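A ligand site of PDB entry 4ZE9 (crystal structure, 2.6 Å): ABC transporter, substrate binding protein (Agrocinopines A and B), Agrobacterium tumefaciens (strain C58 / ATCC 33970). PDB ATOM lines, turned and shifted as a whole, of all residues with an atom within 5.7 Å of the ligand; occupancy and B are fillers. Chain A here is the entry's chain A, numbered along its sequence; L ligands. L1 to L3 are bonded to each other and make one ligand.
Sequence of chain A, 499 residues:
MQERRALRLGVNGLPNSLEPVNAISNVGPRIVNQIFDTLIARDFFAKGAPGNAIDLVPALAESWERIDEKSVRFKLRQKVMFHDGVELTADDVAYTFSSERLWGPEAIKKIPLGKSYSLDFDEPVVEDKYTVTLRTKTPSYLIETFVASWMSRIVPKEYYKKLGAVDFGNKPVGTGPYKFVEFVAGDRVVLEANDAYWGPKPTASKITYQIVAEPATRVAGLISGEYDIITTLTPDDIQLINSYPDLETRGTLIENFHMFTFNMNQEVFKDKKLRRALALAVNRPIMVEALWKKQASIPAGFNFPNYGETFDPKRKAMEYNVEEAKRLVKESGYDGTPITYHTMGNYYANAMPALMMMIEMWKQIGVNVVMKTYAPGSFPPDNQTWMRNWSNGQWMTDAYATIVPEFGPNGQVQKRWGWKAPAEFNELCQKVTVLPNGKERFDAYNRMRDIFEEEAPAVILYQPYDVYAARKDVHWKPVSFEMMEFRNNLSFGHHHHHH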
ATOM      1  N   GLY A  13      32.794  10.776 -22.290  1.00  0.00           N
ATOM      2  CA  GLY A  13      32.983   9.341 -22.415  1.00  0.00           C
ATOM      3  C   GLY A  13      32.174   8.739 -23.542  1.00  0.00           C
ATOM      4  O   GLY A  13      31.407   9.434 -24.228  1.00  0.00           O
ATOM      5  N   LEU A  14      32.342   7.427 -23.734  1.00  0.00           N
ATOM      6  CA  LEU A  14      31.642   6.628 -24.749  1.00  0.00           C
ATOM      7  C   LEU A  14      31.113   5.349 -24.079  1.00  0.00           C
ATOM      8  O   LEU A  14      31.741   4.866 -23.136  1.00  0.00           O
ATOM      9  CB  LEU A  14      32.582   6.273 -25.932  1.00  0.00           C
ATOM     10  CG  LEU A  14      33.193   7.424 -26.753  1.00  0.00           C
ATOM     11  CD1 LEU A  14      34.296   6.923 -27.645  1.00  0.00           C
ATOM     12  CD2 LEU A  14      32.156   8.138 -27.589  1.00  0.00           C
ATOM     13  N   PRO A  15      29.984   4.752 -24.537  1.00  0.00           N
ATOM     14  CA  PRO A  15      29.530   3.500 -23.891  1.00  0.00           C
ATOM     15  C   PRO A  15      30.414   2.339 -24.329  1.00  0.00           C
ATOM     16  O   PRO A  15      31.053   2.433 -25.377  1.00  0.00           O
ATOM     17  CB  PRO A  15      28.091   3.349 -24.399  1.00  0.00           C
ATOM     18  CG  PRO A  15      28.076   4.029 -25.721  1.00  0.00           C
ATOM     19  CD  PRO A  15      29.094   5.146 -25.661  1.00  0.00           C
ATOM     20  N   ASN A  16      30.492   1.265 -23.533  1.00  0.00           N
ATOM     21  CA  ASN A  16      31.291   0.080 -23.876  1.00  0.00           C
ATOM     22  C   ASN A  16      30.589  -0.706 -24.985  1.00  0.00           C
ATOM     23  O   ASN A  16      31.240  -1.475 -25.708  1.00  0.00           O
ATOM     24  CB  ASN A  16      31.525  -0.802 -22.644  1.00  0.00           C
ATOM     25  CG  ASN A  16      32.297  -0.132 -21.525  1.00  0.00           C
ATOM     26  OD1 ASN A  16      31.873  -0.155 -20.370  1.00  0.00           O
ATOM     27  ND2 ASN A  16      33.452   0.440 -21.837  1.00  0.00           N
ATOM     28  N   SER A  17      29.267  -0.493 -25.141  1.00  0.00           N
ATOM     29  CA  SER A  17      28.442  -1.130 -26.163  1.00  0.00           C
ATOM     30  C   SER A  17      27.419  -0.165 -26.768  1.00  0.00           C
ATOM     31  O   SER A  17      26.865   0.683 -26.072  1.00  0.00           O
ATOM     32  CB  SER A  17      27.711  -2.330 -25.586  1.00  0.00           C
ATOM     33  OG  SER A  17      26.869  -2.899 -26.577  1.00  0.00           O
ATOM     34  N   ASN A  22      22.188  -1.940 -23.182  1.00  0.00           N
ATOM     35  CA  ASN A  22      23.532  -1.978 -22.617  1.00  0.00           C
ATOM     36  C   ASN A  22      24.228  -0.615 -22.633  1.00  0.00           C
ATOM     37  O   ASN A  22      25.147  -0.397 -21.852  1.00  0.00           O
ATOM     38  CB  ASN A  22      24.390  -3.050 -23.271  1.00  0.00           C
ATOM     39  CG  ASN A  22      23.925  -4.458 -22.983  1.00  0.00           C
ATOM     40  OD1 ASN A  22      23.941  -5.331 -23.852  1.00  0.00           O
ATOM     41  ND2 ASN A  22      23.463  -4.699 -21.769  1.00  0.00           N
ATOM     42  N   ALA A  23      23.748   0.307 -23.498  1.00  0.00           N
ATOM     43  CA  ALA A  23      24.263   1.667 -23.660  1.00  0.00           C
ATOM     44  C   ALA A  23      23.693   2.659 -22.627  1.00  0.00           C
ATOM     45  O   ALA A  23      24.205   3.770 -22.543  1.00  0.00           O
ATOM     46  CB  ALA A  23      23.994   2.153 -25.075  1.00  0.00           C
ATOM     47  N   ILE A  24      22.651   2.268 -21.852  1.00  0.00           N
ATOM     48  CA  ILE A  24      22.038   3.108 -20.812  1.00  0.00           C
ATOM     49  C   ILE A  24      23.125   3.601 -19.841  1.00  0.00           C
ATOM     50  O   ILE A  24      23.721   2.811 -19.104  1.00  0.00           O
ATOM     51  CB  ILE A  24      20.847   2.408 -20.098  1.00  0.00           C
ATOM     52  CG1 ILE A  24      19.632   2.347 -21.029  1.00  0.00           C
ATOM     53  CG2 ILE A  24      20.508   3.060 -18.738  1.00  0.00           C
ATOM     54  CD1 ILE A  24      18.666   1.294 -20.713  1.00  0.00           C
ATOM     55  N   SER A  25      23.420   4.909 -19.938  1.00  0.00           N
ATOM     56  CA  SER A  25      24.452   5.618 -19.177  1.00  0.00           C
ATOM     57  C   SER A  25      24.322   7.121 -19.468  1.00  0.00           C
ATOM     58  O   SER A  25      23.385   7.527 -20.165  1.00  0.00           O
ATOM     59  CB  SER A  25      25.841   5.135 -19.583  1.00  0.00           C
ATOM     60  OG  SER A  25      26.014   5.137 -20.987  1.00  0.00           O
ATOM     61  N   ASN A  26      25.245   7.954 -18.942  1.00  0.00           N
ATOM     62  CA  ASN A  26      25.209   9.385 -19.240  1.00  0.00           C
ATOM     63  C   ASN A  26      25.801   9.628 -20.647  1.00  0.00           C
ATOM     64  O   ASN A  26      25.556  10.683 -21.245  1.00  0.00           O
ATOM     65  CB  ASN A  26      26.020  10.195 -18.197  1.00  0.00           C
ATOM     66  CG  ASN A  26      25.392  10.317 -16.820  1.00  0.00           C
ATOM     67  OD1 ASN A  26      24.397   9.662 -16.462  1.00  0.00           O
ATOM     68  ND2 ASN A  26      25.985  11.156 -15.994  1.00  0.00           N
ATOM     69  N   VAL A  27      26.545   8.634 -21.183  1.00  0.00           N
ATOM     70  CA  VAL A  27      27.253   8.737 -22.463  1.00  0.00           C
ATOM     71  C   VAL A  27      26.704   7.980 -23.677  1.00  0.00           C
ATOM     72  O   VAL A  27      27.034   8.330 -24.804  1.00  0.00           O
ATOM     73  CB  VAL A  27      28.763   8.513 -22.269  1.00  0.00           C
ATOM     74  CG1 VAL A  27      29.371   9.616 -21.424  1.00  0.00           C
ATOM     75  CG2 VAL A  27      29.049   7.139 -21.662  1.00  0.00           C
ATOM     76  N   TYR A 117      15.470  -3.906 -15.056  1.00  0.00           N
ATOM     77  CA  TYR A 117      14.982  -2.632 -15.580  1.00  0.00           C
ATOM     78  C   TYR A 117      13.621  -2.792 -16.258  1.00  0.00           C
ATOM     79  O   TYR A 117      12.952  -1.798 -16.493  1.00  0.00           O
ATOM     80  CB  TYR A 117      15.989  -2.037 -16.571  1.00  0.00           C
ATOM     81  CG  TYR A 117      17.263  -1.454 -16.003  1.00  0.00           C
ATOM     82  CD1 TYR A 117      17.580  -1.585 -14.658  1.00  0.00           C
ATOM     83  CD2 TYR A 117      18.181  -0.797 -16.827  1.00  0.00           C
ATOM     84  CE1 TYR A 117      18.758  -1.073 -14.137  1.00  0.00           C
ATOM     85  CE2 TYR A 117      19.365  -0.263 -16.311  1.00  0.00           C
ATOM     86  CZ  TYR A 117      19.657  -0.411 -14.967  1.00  0.00           C
ATOM     87  OH  TYR A 117      20.817   0.105 -14.451  1.00  0.00           O
ATOM     88  N   TRP A 150      14.538   4.848 -22.891  1.00  0.00           N
ATOM     89  CA  TRP A 150      15.798   4.364 -23.437  1.00  0.00           C
ATOM     90  C   TRP A 150      15.896   2.841 -23.417  1.00  0.00           C
ATOM     91  O   TRP A 150      16.854   2.272 -23.931  1.00  0.00           O
ATOM     92  CB  TRP A 150      16.984   5.019 -22.700  1.00  0.00           C
ATOM     93  CG  TRP A 150      16.962   4.909 -21.194  1.00  0.00           C
ATOM     94  CD1 TRP A 150      16.145   4.149 -20.423  1.00  0.00           C
ATOM     95  CD2 TRP A 150      17.850   5.580 -20.295  1.00  0.00           C
ATOM     96  NE1 TRP A 150      16.460   4.295 -19.105  1.00  0.00           N
ATOM     97  CE2 TRP A 150      17.493   5.198 -18.990  1.00  0.00           C
ATOM     98  CE3 TRP A 150      18.905   6.482 -20.473  1.00  0.00           C
ATOM     99  CZ2 TRP A 150      18.170   5.670 -17.859  1.00  0.00           C
ATOM    100  CZ3 TRP A 150      19.549   6.982 -19.358  1.00  0.00           C
ATOM    101  CH2 TRP A 150      19.171   6.586 -18.063  1.00  0.00           C
ATOM    102  N   ASN A 256      17.976  13.652 -13.931  1.00  0.00           N
ATOM    103  CA  ASN A 256      19.027  12.775 -13.437  1.00  0.00           C
ATOM    104  C   ASN A 256      19.483  13.276 -12.073  1.00  0.00           C
ATOM    105  O   ASN A 256      19.322  14.457 -11.777  1.00  0.00           O
ATOM    106  CB  ASN A 256      20.211  12.765 -14.423  1.00  0.00           C
ATOM    107  CG  ASN A 256      21.453  12.014 -13.990  1.00  0.00           C
ATOM    108  OD1 ASN A 256      22.234  12.484 -13.147  1.00  0.00           O
ATOM    109  ND2 ASN A 256      21.664  10.854 -14.554  1.00  0.00           N
ATOM    110  N   MET A 344      35.708   8.010 -11.824  1.00  0.00           N
ATOM    111  CA  MET A 344      36.310   7.897 -13.142  1.00  0.00           C
ATOM    112  C   MET A 344      36.596   9.319 -13.604  1.00  0.00           C
ATOM    113  O   MET A 344      35.834   9.866 -14.406  1.00  0.00           O
ATOM    114  CB  MET A 344      35.335   7.207 -14.085  1.00  0.00           C
ATOM    115  CG  MET A 344      35.992   6.612 -15.295  1.00  0.00           C
ATOM    116  SD  MET A 344      34.650   5.734 -16.303  1.00  0.00           S
ATOM    117  CE  MET A 344      34.613   6.969 -17.793  1.00  0.00           C
ATOM    118  N   TYR A 347      33.947  12.014 -15.325  1.00  0.00           N
ATOM    119  CA  TYR A 347      32.939  11.398 -16.177  1.00  0.00           C
ATOM    120  C   TYR A 347      31.628  12.119 -15.844  1.00  0.00           C
ATOM    121  O   TYR A 347      30.887  12.522 -16.745  1.00  0.00           O
ATOM    122  CB  TYR A 347      32.859   9.884 -15.903  1.00  0.00           C
ATOM    123  CG  TYR A 347      31.679   9.176 -16.552  1.00  0.00           C
ATOM    124  CD1 TYR A 347      31.750   8.698 -17.856  1.00  0.00           C
ATOM    125  CD2 TYR A 347      30.511   8.928 -15.831  1.00  0.00           C
ATOM    126  CE1 TYR A 347      30.682   8.002 -18.444  1.00  0.00           C
ATOM    127  CE2 TYR A 347      29.432   8.251 -16.407  1.00  0.00           C
ATOM    128  CZ  TYR A 347      29.528   7.791 -17.710  1.00  0.00           C
ATOM    129  OH  TYR A 347      28.462   7.106 -18.262  1.00  0.00           O
ATOM    130  N   TYR A 348      31.383  12.324 -14.527  1.00  0.00           N
ATOM    131  CA  TYR A 348      30.277  13.109 -14.017  1.00  0.00           C
ATOM    132  C   TYR A 348      30.860  14.493 -13.776  1.00  0.00           C
ATOM    133  O   TYR A 348      31.950  14.603 -13.220  1.00  0.00           O
ATOM    134  CB  TYR A 348      29.718  12.540 -12.690  1.00  0.00           C
ATOM    135  CG  TYR A 348      29.219  11.115 -12.772  1.00  0.00           C
ATOM    136  CD1 TYR A 348      28.053  10.800 -13.461  1.00  0.00           C
ATOM    137  CD2 TYR A 348      29.885  10.077 -12.117  1.00  0.00           C
ATOM    138  CE1 TYR A 348      27.592   9.489 -13.561  1.00  0.00           C
ATOM    139  CE2 TYR A 348      29.422   8.767 -12.174  1.00  0.00           C
ATOM    140  CZ  TYR A 348      28.271   8.478 -12.896  1.00  0.00           C
ATOM    141  OH  TYR A 348      27.817   7.174 -12.980  1.00  0.00           O
ATOM    142  N   TYR A 374      39.883   5.628 -11.541  1.00  0.00           N
ATOM    143  CA  TYR A 374      39.900   4.502 -12.474  1.00  0.00           C
ATOM    144  C   TYR A 374      39.680   4.944 -13.904  1.00  0.00           C
ATOM    145  O   TYR A 374      38.835   5.802 -14.172  1.00  0.00           O
ATOM    146  CB  TYR A 374      38.961   3.366 -12.049  1.00  0.00           C
ATOM    147  CG  TYR A 374      37.488   3.690 -12.081  1.00  0.00           C
ATOM    148  CD1 TYR A 374      36.709   3.382 -13.189  1.00  0.00           C
ATOM    149  CD2 TYR A 374      36.847   4.233 -10.963  1.00  0.00           C
ATOM    150  CE1 TYR A 374      35.336   3.639 -13.212  1.00  0.00           C
ATOM    151  CE2 TYR A 374      35.472   4.498 -10.974  1.00  0.00           C
ATOM    152  CZ  TYR A 374      34.723   4.201 -12.102  1.00  0.00           C
ATOM    153  OH  TYR A 374      33.383   4.465 -12.124  1.00  0.00           O
ATOM    154  N   PRO A 376      38.603   5.053 -17.945  1.00  0.00           N
ATOM    155  CA  PRO A 376      37.375   4.666 -18.649  1.00  0.00           C
ATOM    156  C   PRO A 376      37.342   3.210 -19.121  1.00  0.00           C
ATOM    157  O   PRO A 376      38.371   2.676 -19.560  1.00  0.00           O
ATOM    158  CB  PRO A 376      37.332   5.616 -19.836  1.00  0.00           C
ATOM    159  CG  PRO A 376      38.059   6.822 -19.370  1.00  0.00           C
ATOM    160  CD  PRO A 376      39.156   6.309 -18.493  1.00  0.00           C
ATOM    161  N   GLY A 377      36.161   2.589 -19.010  1.00  0.00           N
ATOM    162  CA  GLY A 377      35.926   1.209 -19.393  1.00  0.00           C
ATOM    163  C   GLY A 377      35.741   0.277 -18.213  1.00  0.00           C
ATOM    164  O   GLY A 377      36.663  -0.444 -17.825  1.00  0.00           O
ATOM    165  N   PHE A 379      36.386  -0.008 -15.029  1.00  0.00           N
ATOM    166  CA  PHE A 379      35.770  -0.174 -13.710  1.00  0.00           C
ATOM    167  C   PHE A 379      36.522  -1.242 -12.894  1.00  0.00           C
ATOM    168  O   PHE A 379      36.872  -2.276 -13.450  1.00  0.00           O
ATOM    169  CB  PHE A 379      34.262  -0.487 -13.835  1.00  0.00           C
ATOM    170  CG  PHE A 379      33.497  -0.421 -12.538  1.00  0.00           C
ATOM    171  CD1 PHE A 379      33.174  -1.577 -11.838  1.00  0.00           C
ATOM    172  CD2 PHE A 379      33.095   0.801 -12.002  1.00  0.00           C
ATOM    173  CE1 PHE A 379      32.486  -1.511 -10.622  1.00  0.00           C
ATOM    174  CE2 PHE A 379      32.400   0.872 -10.798  1.00  0.00           C
ATOM    175  CZ  PHE A 379      32.101  -0.294 -10.114  1.00  0.00           C
ATOM    176  N   TRP A 390      28.008   7.653  -8.699  1.00  0.00           N
ATOM    177  CA  TRP A 390      27.066   7.099  -9.666  1.00  0.00           C
ATOM    178  C   TRP A 390      25.997   8.144  -9.947  1.00  0.00           C
ATOM    179  O   TRP A 390      26.026   9.233  -9.383  1.00  0.00           O
ATOM    180  CB  TRP A 390      26.450   5.808  -9.070  1.00  0.00           C
ATOM    181  CG  TRP A 390      25.636   4.964 -10.014  1.00  0.00           C
ATOM    182  CD1 TRP A 390      25.792   4.850 -11.363  1.00  0.00           C
ATOM    183  CD2 TRP A 390      24.608   4.041  -9.649  1.00  0.00           C
ATOM    184  NE1 TRP A 390      24.881   3.947 -11.867  1.00  0.00           N
ATOM    185  CE2 TRP A 390      24.143   3.433 -10.835  1.00  0.00           C
ATOM    186  CE3 TRP A 390      24.029   3.664  -8.416  1.00  0.00           C
ATOM    187  CZ2 TRP A 390      23.112   2.491 -10.840  1.00  0.00           C
ATOM    188  CZ3 TRP A 390      23.002   2.733  -8.428  1.00  0.00           C
ATOM    189  CH2 TRP A 390      22.548   2.168  -9.623  1.00  0.00           C
ATOM    190  N   SER A 391      25.083   7.847 -10.872  1.00  0.00           N
ATOM    191  CA  SER A 391      23.983   8.728 -11.231  1.00  0.00           C
ATOM    192  C   SER A 391      22.811   7.865 -11.685  1.00  0.00           C
ATOM    193  O   SER A 391      23.026   6.719 -12.105  1.00  0.00           O
ATOM    194  CB  SER A 391      24.385   9.722 -12.315  1.00  0.00           C
ATOM    195  OG  SER A 391      24.048   9.264 -13.621  1.00  0.00           O
ATOM    196  N   ASN A 392      21.596   8.404 -11.585  1.00  0.00           N
ATOM    197  CA  ASN A 392      20.393   7.710 -12.035  1.00  0.00           C
ATOM    198  C   ASN A 392      19.521   8.641 -12.823  1.00  0.00           C
ATOM    199  O   ASN A 392      19.105   9.696 -12.316  1.00  0.00           O
ATOM    200  CB  ASN A 392      19.593   7.147 -10.861  1.00  0.00           C
ATOM    201  CG  ASN A 392      19.987   5.786 -10.398  1.00  0.00           C
ATOM    202  OD1 ASN A 392      21.019   5.238 -10.786  1.00  0.00           O
ATOM    203  ND2 ASN A 392      19.213   5.252  -9.478  1.00  0.00           N
ATOM    204  N   GLY A 393      19.265   8.260 -14.064  1.00  0.00           N
ATOM    205  CA  GLY A 393      18.395   9.006 -14.945  1.00  0.00           C
ATOM    206  C   GLY A 393      16.979   8.543 -14.685  1.00  0.00           C
ATOM    207  O   GLY A 393      16.719   7.351 -14.778  1.00  0.00           O
ATOM    208  N   TRP A 395      13.974   7.901 -15.902  1.00  0.00           N
ATOM    209  CA  TRP A 395      13.504   7.538 -17.232  1.00  0.00           C
ATOM    210  C   TRP A 395      12.006   7.256 -17.444  1.00  0.00           C
ATOM    211  O   TRP A 395      11.615   6.766 -18.516  1.00  0.00           O
ATOM    212  CB  TRP A 395      14.378   6.410 -17.796  1.00  0.00           C
ATOM    213  CG  TRP A 395      14.496   5.184 -16.911  1.00  0.00           C
ATOM    214  CD1 TRP A 395      15.394   4.984 -15.904  1.00  0.00           C
ATOM    215  CD2 TRP A 395      13.781   3.960 -17.065  1.00  0.00           C
ATOM    216  NE1 TRP A 395      15.228   3.728 -15.378  1.00  0.00           N
ATOM    217  CE2 TRP A 395      14.262   3.068 -16.075  1.00  0.00           C
ATOM    218  CE3 TRP A 395      12.761   3.527 -17.935  1.00  0.00           C
ATOM    219  CZ2 TRP A 395      13.754   1.773 -15.928  1.00  0.00           C
ATOM    220  CZ3 TRP A 395      12.278   2.233 -17.802  1.00  0.00           C
ATOM    221  CH2 TRP A 395      12.752   1.379 -16.795  1.00  0.00           C
ATOM    222  N   THR A 402      13.890   5.543 -10.544  1.00  0.00           N
ATOM    223  CA  THR A 402      14.756   4.363 -10.530  1.00  0.00           C
ATOM    224  C   THR A 402      14.754   3.619  -9.196  1.00  0.00           C
ATOM    225  O   THR A 402      15.492   2.637  -9.043  1.00  0.00           O
ATOM    226  CB  THR A 402      16.193   4.760 -10.905  1.00  0.00           C
ATOM    227  OG1 THR A 402      16.660   5.763 -10.010  1.00  0.00           O
ATOM    228  CG2 THR A 402      16.331   5.197 -12.367  1.00  0.00           C
ATOM    229  N   GLU A 406      16.579   0.047  -9.762  1.00  0.00           N
ATOM    230  CA  GLU A 406      17.920   0.051  -9.156  1.00  0.00           C
ATOM    231  C   GLU A 406      17.944  -0.445  -7.706  1.00  0.00           C
ATOM    232  O   GLU A 406      18.798  -1.268  -7.374  1.00  0.00           O
ATOM    233  CB  GLU A 406      18.632   1.414  -9.264  1.00  0.00           C
ATOM    234  CG  GLU A 406      18.738   1.979 -10.677  1.00  0.00           C
ATOM    235  CD  GLU A 406      19.667   1.307 -11.674  1.00  0.00           C
ATOM    236  OE1 GLU A 406      20.367   0.338 -11.305  1.00  0.00           O
ATOM    237  OE2 GLU A 406      19.703   1.783 -12.829  1.00  0.00           O
ATOM    238  N   GLN A 412      20.096  -4.407  -8.936  1.00  0.00           N
ATOM    239  CA  GLN A 412      21.542  -4.555  -8.725  1.00  0.00           C
ATOM    240  C   GLN A 412      22.097  -4.043  -7.368  1.00  0.00           C
ATOM    241  O   GLN A 412      23.102  -4.564  -6.910  1.00  0.00           O
ATOM    242  CB  GLN A 412      22.346  -3.997  -9.920  1.00  0.00           C
ATOM    243  CG  GLN A 412      22.390  -2.461 -10.018  1.00  0.00           C
ATOM    244  CD  GLN A 412      23.247  -1.985 -11.159  1.00  0.00           C
ATOM    245  OE1 GLN A 412      24.436  -2.327 -11.290  1.00  0.00           O
ATOM    246  NE2 GLN A 412      22.663  -1.146 -12.012  1.00  0.00           N
ATOM    247  N   GLU A 482      19.716  12.997 -20.212  1.00  0.00           N
ATOM    248  CA  GLU A 482      21.099  12.626 -20.521  1.00  0.00           C
ATOM    249  C   GLU A 482      21.209  12.016 -21.937  1.00  0.00           C
ATOM    250  O   GLU A 482      21.650  10.883 -22.108  1.00  0.00           O
ATOM    251  CB  GLU A 482      21.684  11.715 -19.426  1.00  0.00           C
ATOM    252  CG  GLU A 482      20.940  10.408 -19.242  1.00  0.00           C
ATOM    253  CD  GLU A 482      21.188   9.713 -17.932  1.00  0.00           C
ATOM    254  OE1 GLU A 482      22.009   8.771 -17.894  1.00  0.00           O
ATOM    255  OE2 GLU A 482      20.552  10.108 -16.930  1.00  0.00           O
HETATM  256  C1  LIG L   1      30.513   2.241 -17.117  1.00  0.00           C
HETATM  257  C2  LIG L   1      31.884   2.446 -17.726  1.00  0.00           C
HETATM  258  O1  LIG L   1      32.799   2.910 -16.765  1.00  0.00           O
HETATM  259  C3  LIG L   1      31.895   3.293 -18.982  1.00  0.00           C
HETATM  260  O2  LIG L   1      32.926   4.307 -18.930  1.00  0.00           O
HETATM  261  C4  LIG L   1      30.665   3.887 -19.456  1.00  0.00           C
HETATM  262  O3  LIG L   1      30.827   4.291 -20.842  1.00  0.00           O
HETATM  263  C5  LIG L   1      29.355   3.187 -19.136  1.00  0.00           C
HETATM  264  O4  LIG L   1      29.487   2.097 -18.100  1.00  0.00           O
HETATM  265  C6  LIG L   1      28.561   2.684 -20.248  1.00  0.00           C
HETATM  266  O5  LIG L   1      29.089   1.667 -21.042  1.00  0.00           O
HETATM  267  O1  LG2 L   2      30.202   3.286 -16.212  1.00  0.00           O
HETATM  268  C1  LG2 L   2      29.482   3.025 -14.959  1.00  0.00           C
HETATM  269  C2  LG2 L   2      30.464   2.547 -13.919  1.00  0.00           C
HETATM  270  O2  LG2 L   2      31.805   2.924 -14.050  1.00  0.00           O
HETATM  271  C3  LG2 L   2      28.878   4.334 -14.546  1.00  0.00           C
HETATM  272  O3  LG2 L   2      29.711   5.434 -14.777  1.00  0.00           O
HETATM  273  O4  LG2 L   2      28.345   2.203 -15.102  1.00  0.00           O
HETATM  274  C4  LG2 L   2      27.209   3.012 -15.241  1.00  0.00           C
HETATM  275  C5  LG2 L   2      26.449   2.713 -16.480  1.00  0.00           C
HETATM  276  O5  LG2 L   2      26.773   1.552 -17.180  1.00  0.00           O
HETATM  277  C6  LG2 L   2      27.706   4.396 -15.286  1.00  0.00           C
HETATM  278  O6  LG2 L   2      26.772   5.248 -14.629  1.00  0.00           O
HETATM  279  O7  LG2 L   2      25.413   7.299 -14.437  1.00  0.00           O
HETATM  280  P1  LG2 L   2      25.766   6.229 -15.430  1.00  0.00           P
HETATM  281  O8  LG2 L   2      26.415   6.832 -16.645  1.00  0.00           O
HETATM  282  C1  LG3 L   3      22.173   6.301 -15.776  1.00  0.00           C
HETATM  283  C2  LG3 L   3      23.221   5.398 -15.181  1.00  0.00           C
HETATM  284  C3  LG3 L   3      22.799   4.041 -15.116  1.00  0.00           C
HETATM  285  C4  LG3 L   3      21.490   3.818 -14.587  1.00  0.00           C
HETATM  286  C5  LG3 L   3      20.427   4.811 -15.038  1.00  0.00           C
HETATM  287  O1  LG3 L   3      22.572   7.596 -15.583  1.00  0.00           O
HETATM  288  O2  LG3 L   3      24.465   5.481 -15.945  1.00  0.00           O
HETATM  289  O3  LG3 L   3      23.811   3.272 -14.376  1.00  0.00           O
HETATM  290  O4  LG3 L   3      21.512   3.817 -13.161  1.00  0.00           O
HETATM  291  O5  LG3 L   3      20.898   6.140 -15.179  1.00  0.00           O
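An oxygen (O4) of LG3 L3 is in hydrogen-bond range of the side-chain amide oxygen (OD1) of Asn 392 (2.8 Å).
NE1 of Trp 390 is in hydrogen-bond range of O3 of LG3 L3 (2.8 Å).
The side-chain carboxylate (OE1) of Glu 482 is in hydrogen-bond range of an oxygen (O1) of LG3 L3.
An oxygen (O7) of LG2 L2 is in hydrogen-bond range of the side-chain hydroxyl of Ser 391.
The side-chain hydroxyl (OH) of Tyr 374 lies within hydrogen-bond range of an oxygen (O2) of LG2 L2 (2.9 Å).
The side-chain hydroxyl (OH) of Tyr 348 sits at hydrogen-bond distance from an oxygen (O6) of LG2 L2, at 2.7 Å.
N of Asn 16 sits at hydrogen-bond distance from O5 of LIG L1, at 2.9 Å.
O of Leu 14 sits at hydrogen-bond distance from O3 of LIG L1, at 2.5 Å.
O of Ser 391 sits close to O4 of LG3 L3.
The side-chain carboxylate of Glu 406 is in hydrogen-bond range of an oxygen (O4) of LG3 L3, 2.7 Å away.
An oxygen (O8) of LG2 L2 lies within hydrogen-bond range of the side-chain hydroxyl (OH) of Tyr 347.
An oxygen (O1) of LG3 L3 lies within hydrogen-bond range of the side-chain amide oxygen (OD1) of Asn 26, 2.9 Å away.
The backbone NH of Asn 26 lies within hydrogen-bond range of an oxygen (O8) of LG2 L2 (2.8 Å).
N of Gly 393 is in hydrogen-bond range of O5 of LG3 L3 (2.9 Å).
The side-chain sulfur of Met 344 lies within hydrogen-bond range of an oxygen (O1) of LIG L1 (3.4 Å).
The side-chain amide oxygen (OD1) of Asn 16 sits at hydrogen-bond distance from an oxygen (O5) of LIG L1 (3.4 Å).
Pro 15 touches the ligand.
O of Ile 24 touches C5 of LG2 L2 (3.8 Å).
Ser 25 touches the ligand.
CG2 of Val 27 touches O3 of LIG L1 (3.5 Å).
OH of Tyr 117 touches C4 of LG3 L3, 3.8 Å away.
CH2 of Trp 150 touches O5 of LG3 L3, 3.4 Å away.
ND2 of Asn 256 touches O1 of LG3 L3 (3.5 Å).
Gly 377 touches the ligand.
Phe 379 touches the ligand.
Of the 30 residues printed, 22 come within 4 Å of the ligand.
The side-chain amide oxygen (OD1) of Asn 26 is in hydrogen-bond range of the side-chain hydroxyl (OG) of Ser 391, at 2.9 Å.
OE2 of Glu 406 lies within hydrogen-bond range of OH of Tyr 117 (2.6 Å).
The side-chain carboxylate (OE2) of Glu 482 is in hydrogen-bond range of the side-chain amide nitrogen (ND2) of Asn 256 (2.7 Å).
NE2 of Gln 412 is in hydrogen-bond range of OH of Tyr 117, at 3.3 Å.
The side-chain carboxylate (OE1) of Glu 482 lies close to the side-chain amide oxygen (OD1) of Asn 26 (2.9 Å).
OE1 of Glu 406 is in hydrogen-bond range of NE2 of Gln 412 (2.8 Å).
The backbone NH (N) of Asn 26 is in hydrogen-bond range of the side-chain hydroxyl (OH) of Tyr 347 (3.4 Å).
OG of Ser 391 lies within hydrogen-bond range of ND2 of Asn 256, at 3.0 Å.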
